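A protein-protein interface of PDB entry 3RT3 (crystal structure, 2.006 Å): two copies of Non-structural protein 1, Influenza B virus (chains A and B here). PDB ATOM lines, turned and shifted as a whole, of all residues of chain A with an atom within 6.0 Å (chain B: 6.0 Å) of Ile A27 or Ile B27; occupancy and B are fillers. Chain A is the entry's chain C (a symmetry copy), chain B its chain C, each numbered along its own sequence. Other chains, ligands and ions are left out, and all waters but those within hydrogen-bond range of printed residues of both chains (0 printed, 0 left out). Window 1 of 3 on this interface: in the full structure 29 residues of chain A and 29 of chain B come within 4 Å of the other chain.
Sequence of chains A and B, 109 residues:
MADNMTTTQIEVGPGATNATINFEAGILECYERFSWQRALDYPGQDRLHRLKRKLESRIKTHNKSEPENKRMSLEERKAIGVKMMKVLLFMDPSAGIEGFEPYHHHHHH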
ATOM      1  N   ASN A  22     -26.990  -4.368  28.054  1.00  0.00           N
ATOM      2  CA  ASN A  22     -26.232  -3.144  28.267  1.00  0.00           C
ATOM      3  C   ASN A  22     -25.675  -2.588  26.956  1.00  0.00           C
ATOM      4  O   ASN A  22     -25.807  -1.391  26.666  1.00  0.00           O
ATOM      5  CB  ASN A  22     -25.126  -3.373  29.294  1.00  0.00           C
ATOM      6  CG  ASN A  22     -25.678  -3.564  30.697  1.00  0.00           C
ATOM      7  OD1 ASN A  22     -26.789  -3.138  30.989  1.00  0.00           O
ATOM      8  ND2 ASN A  22     -24.907  -4.206  31.565  1.00  0.00           N
ATOM      9  N   PHE A  23     -25.071  -3.466  26.161  1.00  0.00           N
ATOM     10  CA  PHE A  23     -24.568  -3.084  24.845  1.00  0.00           C
ATOM     11  C   PHE A  23     -25.658  -2.409  23.999  1.00  0.00           C
ATOM     12  O   PHE A  23     -25.427  -1.384  23.376  1.00  0.00           O
ATOM     13  CB  PHE A  23     -24.026  -4.306  24.102  1.00  0.00           C
ATOM     14  CG  PHE A  23     -23.649  -4.025  22.667  1.00  0.00           C
ATOM     15  CD1 PHE A  23     -22.511  -3.277  22.362  1.00  0.00           C
ATOM     16  CD2 PHE A  23     -24.430  -4.510  21.622  1.00  0.00           C
ATOM     17  CE1 PHE A  23     -22.149  -3.010  21.023  1.00  0.00           C
ATOM     18  CE2 PHE A  23     -24.076  -4.257  20.293  1.00  0.00           C
ATOM     19  CZ  PHE A  23     -22.932  -3.504  20.003  1.00  0.00           C
ATOM     20  N   GLU A  24     -26.851  -2.984  23.979  1.00  0.00           N
ATOM     21  CA  GLU A  24     -27.884  -2.453  23.103  1.00  0.00           C
ATOM     22  C   GLU A  24     -28.544  -1.190  23.661  1.00  0.00           C
ATOM     23  O   GLU A  24     -29.102  -0.386  22.908  1.00  0.00           O
ATOM     24  CB  GLU A  24     -28.890  -3.534  22.719  1.00  0.00           C
ATOM     25  CG  GLU A  24     -28.314  -4.546  21.746  1.00  0.00           C
ATOM     26  CD  GLU A  24     -29.317  -5.597  21.337  1.00  0.00           C
ATOM     27  OE1 GLU A  24     -29.930  -6.192  22.234  1.00  0.00           O
ATOM     28  OE2 GLU A  24     -29.490  -5.837  20.127  1.00  0.00           O
ATOM     29  N   ALA A  25     -28.464  -1.005  24.975  1.00  0.00           N
ATOM     30  CA  ALA A  25     -28.809   0.274  25.565  1.00  0.00           C
ATOM     31  C   ALA A  25     -27.865   1.346  25.014  1.00  0.00           C
ATOM     32  O   ALA A  25     -28.272   2.471  24.767  1.00  0.00           O
ATOM     33  CB  ALA A  25     -28.733   0.211  27.100  1.00  0.00           C
ATOM     34  N   GLY A  26     -26.602   0.991  24.823  1.00  0.00           N
ATOM     35  CA  GLY A  26     -25.646   1.926  24.251  1.00  0.00           C
ATOM     36  C   GLY A  26     -25.974   2.167  22.790  1.00  0.00           C
ATOM     37  O   GLY A  26     -25.796   3.268  22.264  1.00  0.00           O
ATOM     38  N   ILE A  27     -26.437   1.115  22.125  1.00  0.00           N
ATOM     39  CA  ILE A  27     -26.827   1.224  20.726  1.00  0.00           C
ATOM     40  C   ILE A  27     -27.990   2.199  20.606  1.00  0.00           C
ATOM     41  O   ILE A  27     -27.995   3.081  19.732  1.00  0.00           O
ATOM     42  CB  ILE A  27     -27.163  -0.158  20.105  1.00  0.00           C
ATOM     43  CG1 ILE A  27     -25.873  -0.965  19.885  1.00  0.00           C
ATOM     44  CG2 ILE A  27     -27.894   0.008  18.778  1.00  0.00           C
ATOM     45  CD1 ILE A  27     -24.950  -0.338  18.892  1.00  0.00           C
ATOM     46  N   LEU A  28     -28.957   2.060  21.500  1.00  0.00           N
ATOM     47  CA  LEU A  28     -30.092   2.970  21.530  1.00  0.00           C
ATOM     48  C   LEU A  28     -29.606   4.418  21.701  1.00  0.00           C
ATOM     49  O   LEU A  28     -30.063   5.322  21.002  1.00  0.00           O
ATOM     50  CB  LEU A  28     -31.050   2.587  22.660  1.00  0.00           C
ATOM     51  CG  LEU A  28     -32.188   3.573  22.920  1.00  0.00           C
ATOM     52  CD1 LEU A  28     -33.075   3.677  21.706  1.00  0.00           C
ATOM     53  CD2 LEU A  28     -32.998   3.106  24.113  1.00  0.00           C
ATOM     54  N   GLU A  29     -28.683   4.633  22.630  1.00  0.00           N
ATOM     55  CA  GLU A  29     -28.146   5.972  22.847  1.00  0.00           C
ATOM     56  C   GLU A  29     -27.598   6.548  21.535  1.00  0.00           C
ATOM     57  O   GLU A  29     -27.833   7.703  21.222  1.00  0.00           O
ATOM     58  CB  GLU A  29     -27.062   5.966  23.925  1.00  0.00           C
ATOM     59  CG  GLU A  29     -26.462   7.342  24.237  1.00  0.00           C
ATOM     60  CD  GLU A  29     -27.470   8.313  24.833  1.00  0.00           C
ATOM     61  OE1 GLU A  29     -27.257   9.538  24.733  1.00  0.00           O
ATOM     62  OE2 GLU A  29     -28.469   7.856  25.416  1.00  0.00           O
ATOM     63  N   CYS A  30     -26.863   5.739  20.781  1.00  0.00           N
ATOM     64  CA  CYS A  30     -26.289   6.185  19.514  1.00  0.00           C
ATOM     65  C   CYS A  30     -27.354   6.587  18.497  1.00  0.00           C
ATOM     66  O   CYS A  30     -27.228   7.623  17.843  1.00  0.00           O
ATOM     67  CB  CYS A  30     -25.407   5.103  18.920  1.00  0.00           C
ATOM     68  SG  CYS A  30     -23.885   4.949  19.857  1.00  0.00           S
ATOM     69  N   TYR A  31     -28.376   5.746  18.358  1.00  0.00           N
ATOM     70  CA  TYR A  31     -29.516   6.050  17.504  1.00  0.00           C
ATOM     71  C   TYR A  31     -30.128   7.354  17.936  1.00  0.00           C
ATOM     72  O   TYR A  31     -30.484   8.181  17.111  1.00  0.00           O
ATOM     73  CB  TYR A  31     -30.580   4.957  17.615  1.00  0.00           C
ATOM     74  CG  TYR A  31     -30.433   3.840  16.608  1.00  0.00           C
ATOM     75  CD1 TYR A  31     -29.600   2.751  16.860  1.00  0.00           C
ATOM     76  CD2 TYR A  31     -31.141   3.865  15.403  1.00  0.00           C
ATOM     77  CE1 TYR A  31     -29.457   1.724  15.928  1.00  0.00           C
ATOM     78  CE2 TYR A  31     -31.001   2.839  14.467  1.00  0.00           C
ATOM     79  CZ  TYR A  31     -30.165   1.772  14.737  1.00  0.00           C
ATOM     80  OH  TYR A  31     -30.025   0.752  13.819  1.00  0.00           O
ATOM     81  N   GLU A  32     -30.293   7.530  19.243  1.00  0.00           N
ATOM     82  CA  GLU A  32     -30.940   8.750  19.721  1.00  0.00           C
ATOM     83  C   GLU A  32     -30.075   9.959  19.383  1.00  0.00           C
ATOM     84  O   GLU A  32     -30.583  10.959  18.892  1.00  0.00           O
ATOM     85  CB  GLU A  32     -31.237   8.681  21.222  1.00  0.00           C
ATOM     86  CG  GLU A  32     -32.355   7.708  21.575  1.00  0.00           C
ATOM     87  CD  GLU A  32     -32.734   7.747  23.044  1.00  0.00           C
ATOM     88  OE1 GLU A  32     -31.942   8.280  23.854  1.00  0.00           O
ATOM     89  OE2 GLU A  32     -33.830   7.247  23.387  1.00  0.00           O
ATOM     90  N   LEU A  51     -36.593  -0.479  19.436  1.00  0.00           N
ATOM     91  CA  LEU A  51     -35.481  -0.958  20.236  1.00  0.00           C
ATOM     92  C   LEU A  51     -35.781  -0.550  21.656  1.00  0.00           C
ATOM     93  O   LEU A  51     -35.670  -1.349  22.582  1.00  0.00           O
ATOM     94  CB  LEU A  51     -34.178  -0.295  19.817  1.00  0.00           C
ATOM     95  CG  LEU A  51     -32.837  -1.046  19.745  1.00  0.00           C
ATOM     96  CD1 LEU A  51     -31.677  -0.072  19.960  1.00  0.00           C
ATOM     97  CD2 LEU A  51     -32.731  -2.226  20.699  1.00  0.00           C
ATOM     98  N   GLY A  81     -23.381   0.939  28.373  1.00  0.00           N
ATOM     99  CA  GLY A  81     -23.360   0.683  26.949  1.00  0.00           C
ATOM    100  C   GLY A  81     -22.460   1.627  26.178  1.00  0.00           C
ATOM    101  O   GLY A  81     -21.708   1.199  25.333  1.00  0.00           O
ATOM    102  N   MET A  85     -19.120   0.756  23.977  1.00  0.00           N
ATOM    103  CA  MET A  85     -18.905   1.090  22.588  1.00  0.00           C
ATOM    104  C   MET A  85     -17.626   1.850  22.361  1.00  0.00           C
ATOM    105  O   MET A  85     -16.973   1.652  21.366  1.00  0.00           O
ATOM    106  CB  MET A  85     -20.117   1.794  21.989  1.00  0.00           C
ATOM    107  CG  MET A  85     -21.110   0.750  21.460  1.00  0.00           C
ATOM    108  SD  MET A  85     -22.655   1.560  21.250  1.00  0.00           S
ATOM    109  CE  MET A  85     -22.079   2.777  20.096  1.00  0.00           C
ATOM    110  N   ASN B  22     -25.221   4.483   6.262  1.00  0.00           N
ATOM    111  CA  ASN B  22     -23.849   4.550   6.746  1.00  0.00           C
ATOM    112  C   ASN B  22     -23.776   4.376   8.263  1.00  0.00           C
ATOM    113  O   ASN B  22     -22.968   3.590   8.776  1.00  0.00           O
ATOM    114  CB  ASN B  22     -23.188   5.851   6.297  1.00  0.00           C
ATOM    115  CG  ASN B  22     -22.918   5.871   4.802  1.00  0.00           C
ATOM    116  OD1 ASN B  22     -22.834   4.822   4.174  1.00  0.00           O
ATOM    117  ND2 ASN B  22     -22.787   7.060   4.230  1.00  0.00           N
ATOM    118  N   PHE B  23     -24.637   5.099   8.974  1.00  0.00           N
ATOM    119  CA  PHE B  23     -24.728   4.966  10.426  1.00  0.00           C
ATOM    120  C   PHE B  23     -24.936   3.504  10.846  1.00  0.00           C
ATOM    121  O   PHE B  23     -24.287   3.012  11.757  1.00  0.00           O
ATOM    122  CB  PHE B  23     -25.870   5.825  10.971  1.00  0.00           C
ATOM    123  CG  PHE B  23     -26.142   5.607  12.441  1.00  0.00           C
ATOM    124  CD1 PHE B  23     -25.257   6.086  13.409  1.00  0.00           C
ATOM    125  CD2 PHE B  23     -27.283   4.926  12.856  1.00  0.00           C
ATOM    126  CE1 PHE B  23     -25.504   5.890  14.785  1.00  0.00           C
ATOM    127  CE2 PHE B  23     -27.539   4.733  14.218  1.00  0.00           C
ATOM    128  CZ  PHE B  23     -26.642   5.218  15.176  1.00  0.00           C
ATOM    129  N   GLU B  24     -25.842   2.806  10.178  1.00  0.00           N
ATOM    130  CA  GLU B  24     -26.162   1.454  10.611  1.00  0.00           C
ATOM    131  C   GLU B  24     -25.111   0.429  10.181  1.00  0.00           C
ATOM    132  O   GLU B  24     -24.982  -0.636  10.793  1.00  0.00           O
ATOM    133  CB  GLU B  24     -27.580   1.065  10.201  1.00  0.00           C
ATOM    134  CG  GLU B  24     -28.639   1.784  11.015  1.00  0.00           C
ATOM    135  CD  GLU B  24     -30.042   1.376  10.637  1.00  0.00           C
ATOM    136  OE1 GLU B  24     -30.350   1.411   9.438  1.00  0.00           O
ATOM    137  OE2 GLU B  24     -30.837   1.028  11.529  1.00  0.00           O
ATOM    138  N   ALA B  25     -24.346   0.756   9.144  1.00  0.00           N
ATOM    139  CA  ALA B  25     -23.155  -0.010   8.831  1.00  0.00           C
ATOM    140  C   ALA B  25     -22.182   0.081  10.010  1.00  0.00           C
ATOM    141  O   ALA B  25     -21.511  -0.884  10.343  1.00  0.00           O
ATOM    142  CB  ALA B  25     -22.498   0.498   7.536  1.00  0.00           C
ATOM    143  N   GLY B  26     -22.110   1.246  10.638  1.00  0.00           N
ATOM    144  CA  GLY B  26     -21.256   1.409  11.804  1.00  0.00           C
ATOM    145  C   GLY B  26     -21.822   0.625  12.971  1.00  0.00           C
ATOM    146  O   GLY B  26     -21.088   0.078  13.796  1.00  0.00           O
ATOM    147  N   ILE B  27     -23.147   0.593  13.051  1.00  0.00           N
ATOM    148  CA  ILE B  27     -23.818  -0.160  14.102  1.00  0.00           C
ATOM    149  C   ILE B  27     -23.483  -1.637  13.951  1.00  0.00           C
ATOM    150  O   ILE B  27     -23.147  -2.319  14.933  1.00  0.00           O
ATOM    151  CB  ILE B  27     -25.349   0.090  14.111  1.00  0.00           C
ATOM    152  CG1 ILE B  27     -25.652   1.495  14.655  1.00  0.00           C
ATOM    153  CG2 ILE B  27     -26.062  -0.952  14.965  1.00  0.00           C
ATOM    154  CD1 ILE B  27     -25.250   1.673  16.082  1.00  0.00           C
ATOM    155  N   LEU B  28     -23.545  -2.122  12.720  1.00  0.00           N
ATOM    156  CA  LEU B  28     -23.186  -3.503  12.436  1.00  0.00           C
ATOM    157  C   LEU B  28     -21.747  -3.783  12.896  1.00  0.00           C
ATOM    158  O   LEU B  28     -21.476  -4.800  13.534  1.00  0.00           O
ATOM    159  CB  LEU B  28     -23.340  -3.795  10.942  1.00  0.00           C
ATOM    160  CG  LEU B  28     -22.819  -5.154  10.479  1.00  0.00           C
ATOM    161  CD1 LEU B  28     -23.588  -6.263  11.151  1.00  0.00           C
ATOM    162  CD2 LEU B  28     -22.960  -5.265   8.974  1.00  0.00           C
ATOM    163  N   GLU B  29     -20.829  -2.881  12.569  1.00  0.00           N
ATOM    164  CA  GLU B  29     -19.441  -3.053  12.983  1.00  0.00           C
ATOM    165  C   GLU B  29     -19.354  -3.244  14.502  1.00  0.00           C
ATOM    166  O   GLU B  29     -18.628  -4.100  14.977  1.00  0.00           O
ATOM    167  CB  GLU B  29     -18.581  -1.867  12.542  1.00  0.00           C
ATOM    168  CG  GLU B  29     -17.097  -1.980  12.912  1.00  0.00           C
ATOM    169  CD  GLU B  29     -16.393  -3.134  12.217  1.00  0.00           C
ATOM    170  OE1 GLU B  29     -15.354  -3.600  12.728  1.00  0.00           O
ATOM    171  OE2 GLU B  29     -16.865  -3.570  11.152  1.00  0.00           O
ATOM    172  N   CYS B  30     -20.093  -2.437  15.256  1.00  0.00           N
ATOM    173  CA  CYS B  30     -20.085  -2.529  16.713  1.00  0.00           C
ATOM    174  C   CYS B  30     -20.585  -3.881  17.217  1.00  0.00           C
ATOM    175  O   CYS B  30     -19.979  -4.473  18.112  1.00  0.00           O
ATOM    176  CB  CYS B  30     -20.925  -1.423  17.321  1.00  0.00           C
ATOM    177  SG  CYS B  30     -20.094   0.159  17.155  1.00  0.00           S
ATOM    178  N   TYR B  31     -21.702  -4.338  16.656  1.00  0.00           N
ATOM    179  CA  TYR B  31     -22.237  -5.658  16.962  1.00  0.00           C
ATOM    180  C   TYR B  31     -21.190  -6.698  16.671  1.00  0.00           C
ATOM    181  O   TYR B  31     -21.003  -7.627  17.442  1.00  0.00           O
ATOM    182  CB  TYR B  31     -23.465  -5.955  16.100  1.00  0.00           C
ATOM    183  CG  TYR B  31     -24.778  -5.546  16.725  1.00  0.00           C
ATOM    184  CD1 TYR B  31     -25.265  -4.247  16.586  1.00  0.00           C
ATOM    185  CD2 TYR B  31     -25.544  -6.465  17.446  1.00  0.00           C
ATOM    186  CE1 TYR B  31     -26.473  -3.866  17.169  1.00  0.00           C
ATOM    187  CE2 TYR B  31     -26.754  -6.087  18.032  1.00  0.00           C
ATOM    188  CZ  TYR B  31     -27.214  -4.793  17.885  1.00  0.00           C
ATOM    189  OH  TYR B  31     -28.411  -4.414  18.457  1.00  0.00           O
ATOM    190  N   GLU B  32     -20.523  -6.570  15.529  1.00  0.00           N
ATOM    191  CA  GLU B  32     -19.538  -7.584  15.162  1.00  0.00           C
ATOM    192  C   GLU B  32     -18.386  -7.570  16.160  1.00  0.00           C
ATOM    193  O   GLU B  32     -17.962  -8.621  16.624  1.00  0.00           O
ATOM    194  CB  GLU B  32     -19.034  -7.390  13.729  1.00  0.00           C
ATOM    195  CG  GLU B  32     -20.075  -7.726  12.668  1.00  0.00           C
ATOM    196  CD  GLU B  32     -19.525  -7.662  11.255  1.00  0.00           C
ATOM    197  OE1 GLU B  32     -18.445  -7.060  11.059  1.00  0.00           O
ATOM    198  OE2 GLU B  32     -20.174  -8.220  10.341  1.00  0.00           O
ATOM    199  N   LEU B  51     -29.264  -7.685  10.409  1.00  0.00           N
ATOM    200  CA  LEU B  51     -28.908  -6.315  10.090  1.00  0.00           C
ATOM    201  C   LEU B  51     -28.048  -6.384   8.853  1.00  0.00           C
ATOM    202  O   LEU B  51     -28.255  -5.642   7.896  1.00  0.00           O
ATOM    203  CB  LEU B  51     -28.086  -5.688  11.205  1.00  0.00           C
ATOM    204  CG  LEU B  51     -28.258  -4.229  11.660  1.00  0.00           C
ATOM    205  CD1 LEU B  51     -26.949  -3.705  12.254  1.00  0.00           C
ATOM    206  CD2 LEU B  51     -28.767  -3.293  10.574  1.00  0.00           C
ATOM    207  N   GLY B  81     -19.431   4.877   9.022  1.00  0.00           N
ATOM    208  CA  GLY B  81     -20.266   4.639  10.178  1.00  0.00           C
ATOM    209  C   GLY B  81     -19.512   4.699  11.492  1.00  0.00           C
ATOM    210  O   GLY B  81     -19.971   5.304  12.432  1.00  0.00           O
ATOM    211  N   MET B  85     -20.018   7.288  14.621  1.00  0.00           N
ATOM    212  CA  MET B  85     -20.284   6.924  15.993  1.00  0.00           C
ATOM    213  C   MET B  85     -19.304   7.534  16.960  1.00  0.00           C
ATOM    214  O   MET B  85     -19.677   7.902  18.046  1.00  0.00           O
ATOM    215  CB  MET B  85     -20.401   5.413  16.156  1.00  0.00           C
ATOM    216  CG  MET B  85     -21.848   4.977  15.886  1.00  0.00           C
ATOM    217  SD  MET B  85     -21.825   3.245  15.598  1.00  0.00           S
ATOM    218  CE  MET B  85     -21.132   2.797  17.168  1.00  0.00           C
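Of the 14 printed residues of chain B, 6 touch a printed residue of chain A.
Printed residues of chain B that touch a printed residue of chain A: Phe B23, Glu B24, Ile B27, Cys B30, Tyr B31 and Met B85.
Hydrophobic or aromatic side chains of chain A that line the printed part of chain B: Phe A23, Ile A27, Tyr A31 and Met A85.
Among the printed residues, 8 pairs touch across the chains.
Among the printed residues, no Asp or Glu carboxylate lies within 4 Å of a Lys or Arg side-chain nitrogen of the other chain.
CZ of Phe A23 touches O of Cys B30 (3.6 Å).
Phe A23 touches Tyr B31 (CZ to N, 3.7 Å).
CD1 of Ile B27 touches CD1 of Ile A27 (3.5 Å).
Cys A30 touches Phe B23.
Tyr A31 touches Phe B23 (N to CZ, 3.7 Å).
Met A85 touches Met B85.
OH of Tyr A31 is in hydrogen-bond range of OE2 of Glu B24, 2.4 Å away.
OH of Tyr B31 is in hydrogen-bond range of OE2 of Glu A24, at 2.4 Å.
Phe A23 touches Cys B30, and with the chains exchanged Cys A30 touches Phe B23.
Phe A23 touches Tyr B31, and with the chains exchanged Tyr A31 touches Phe B23.
Ile B27 touches its own counterpart, Ile A27.
Met B85 touches its own counterpart, Met A85.
14 positions are printed for both chains.
Of the 8 pairs that touch across the chains among the printed residues, 8 have their exchanged pair printed and touching as well.
The backbone carbonyl oxygen of Gly B26 lies within hydrogen-bond range of the side-chain sulfur of Cys B30 (3.5 Å).
The side-chain sulfur (SG) of Cys A30 lies within hydrogen-bond range of the backbone carbonyl oxygen (O) of Gly A26 (3.5 Å).
Of the printed residues of chain B, Phe A23 touches Cys B30 and Tyr B31.
Of the printed residues of chain B, Ile A27 touches Ile B27 (3.5 Å).
Of the printed residues of chain B, Cys A30 touches Phe B23.
Of the printed residues of chain B, Met A85 touches Met B85 (3.1 Å).
Printed residues of chain A within 4 Å of Phe B23: Cys A30 (3.6 Å) and Tyr A31 (3.7 Å).
Gly B26 touches none of the printed residues of chain A.
Printed residues of chain A within 4 Å of Ile B27: Ile A27 (3.5 Å).
Printed residues of chain A within 4 Å of Tyr B31: Phe A23 (3.7 Å) and Glu A24 (2.4 Å).
The nearest printed residue of chain B that does not touch Ile A27 is Tyr B31 (4.02 Å).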
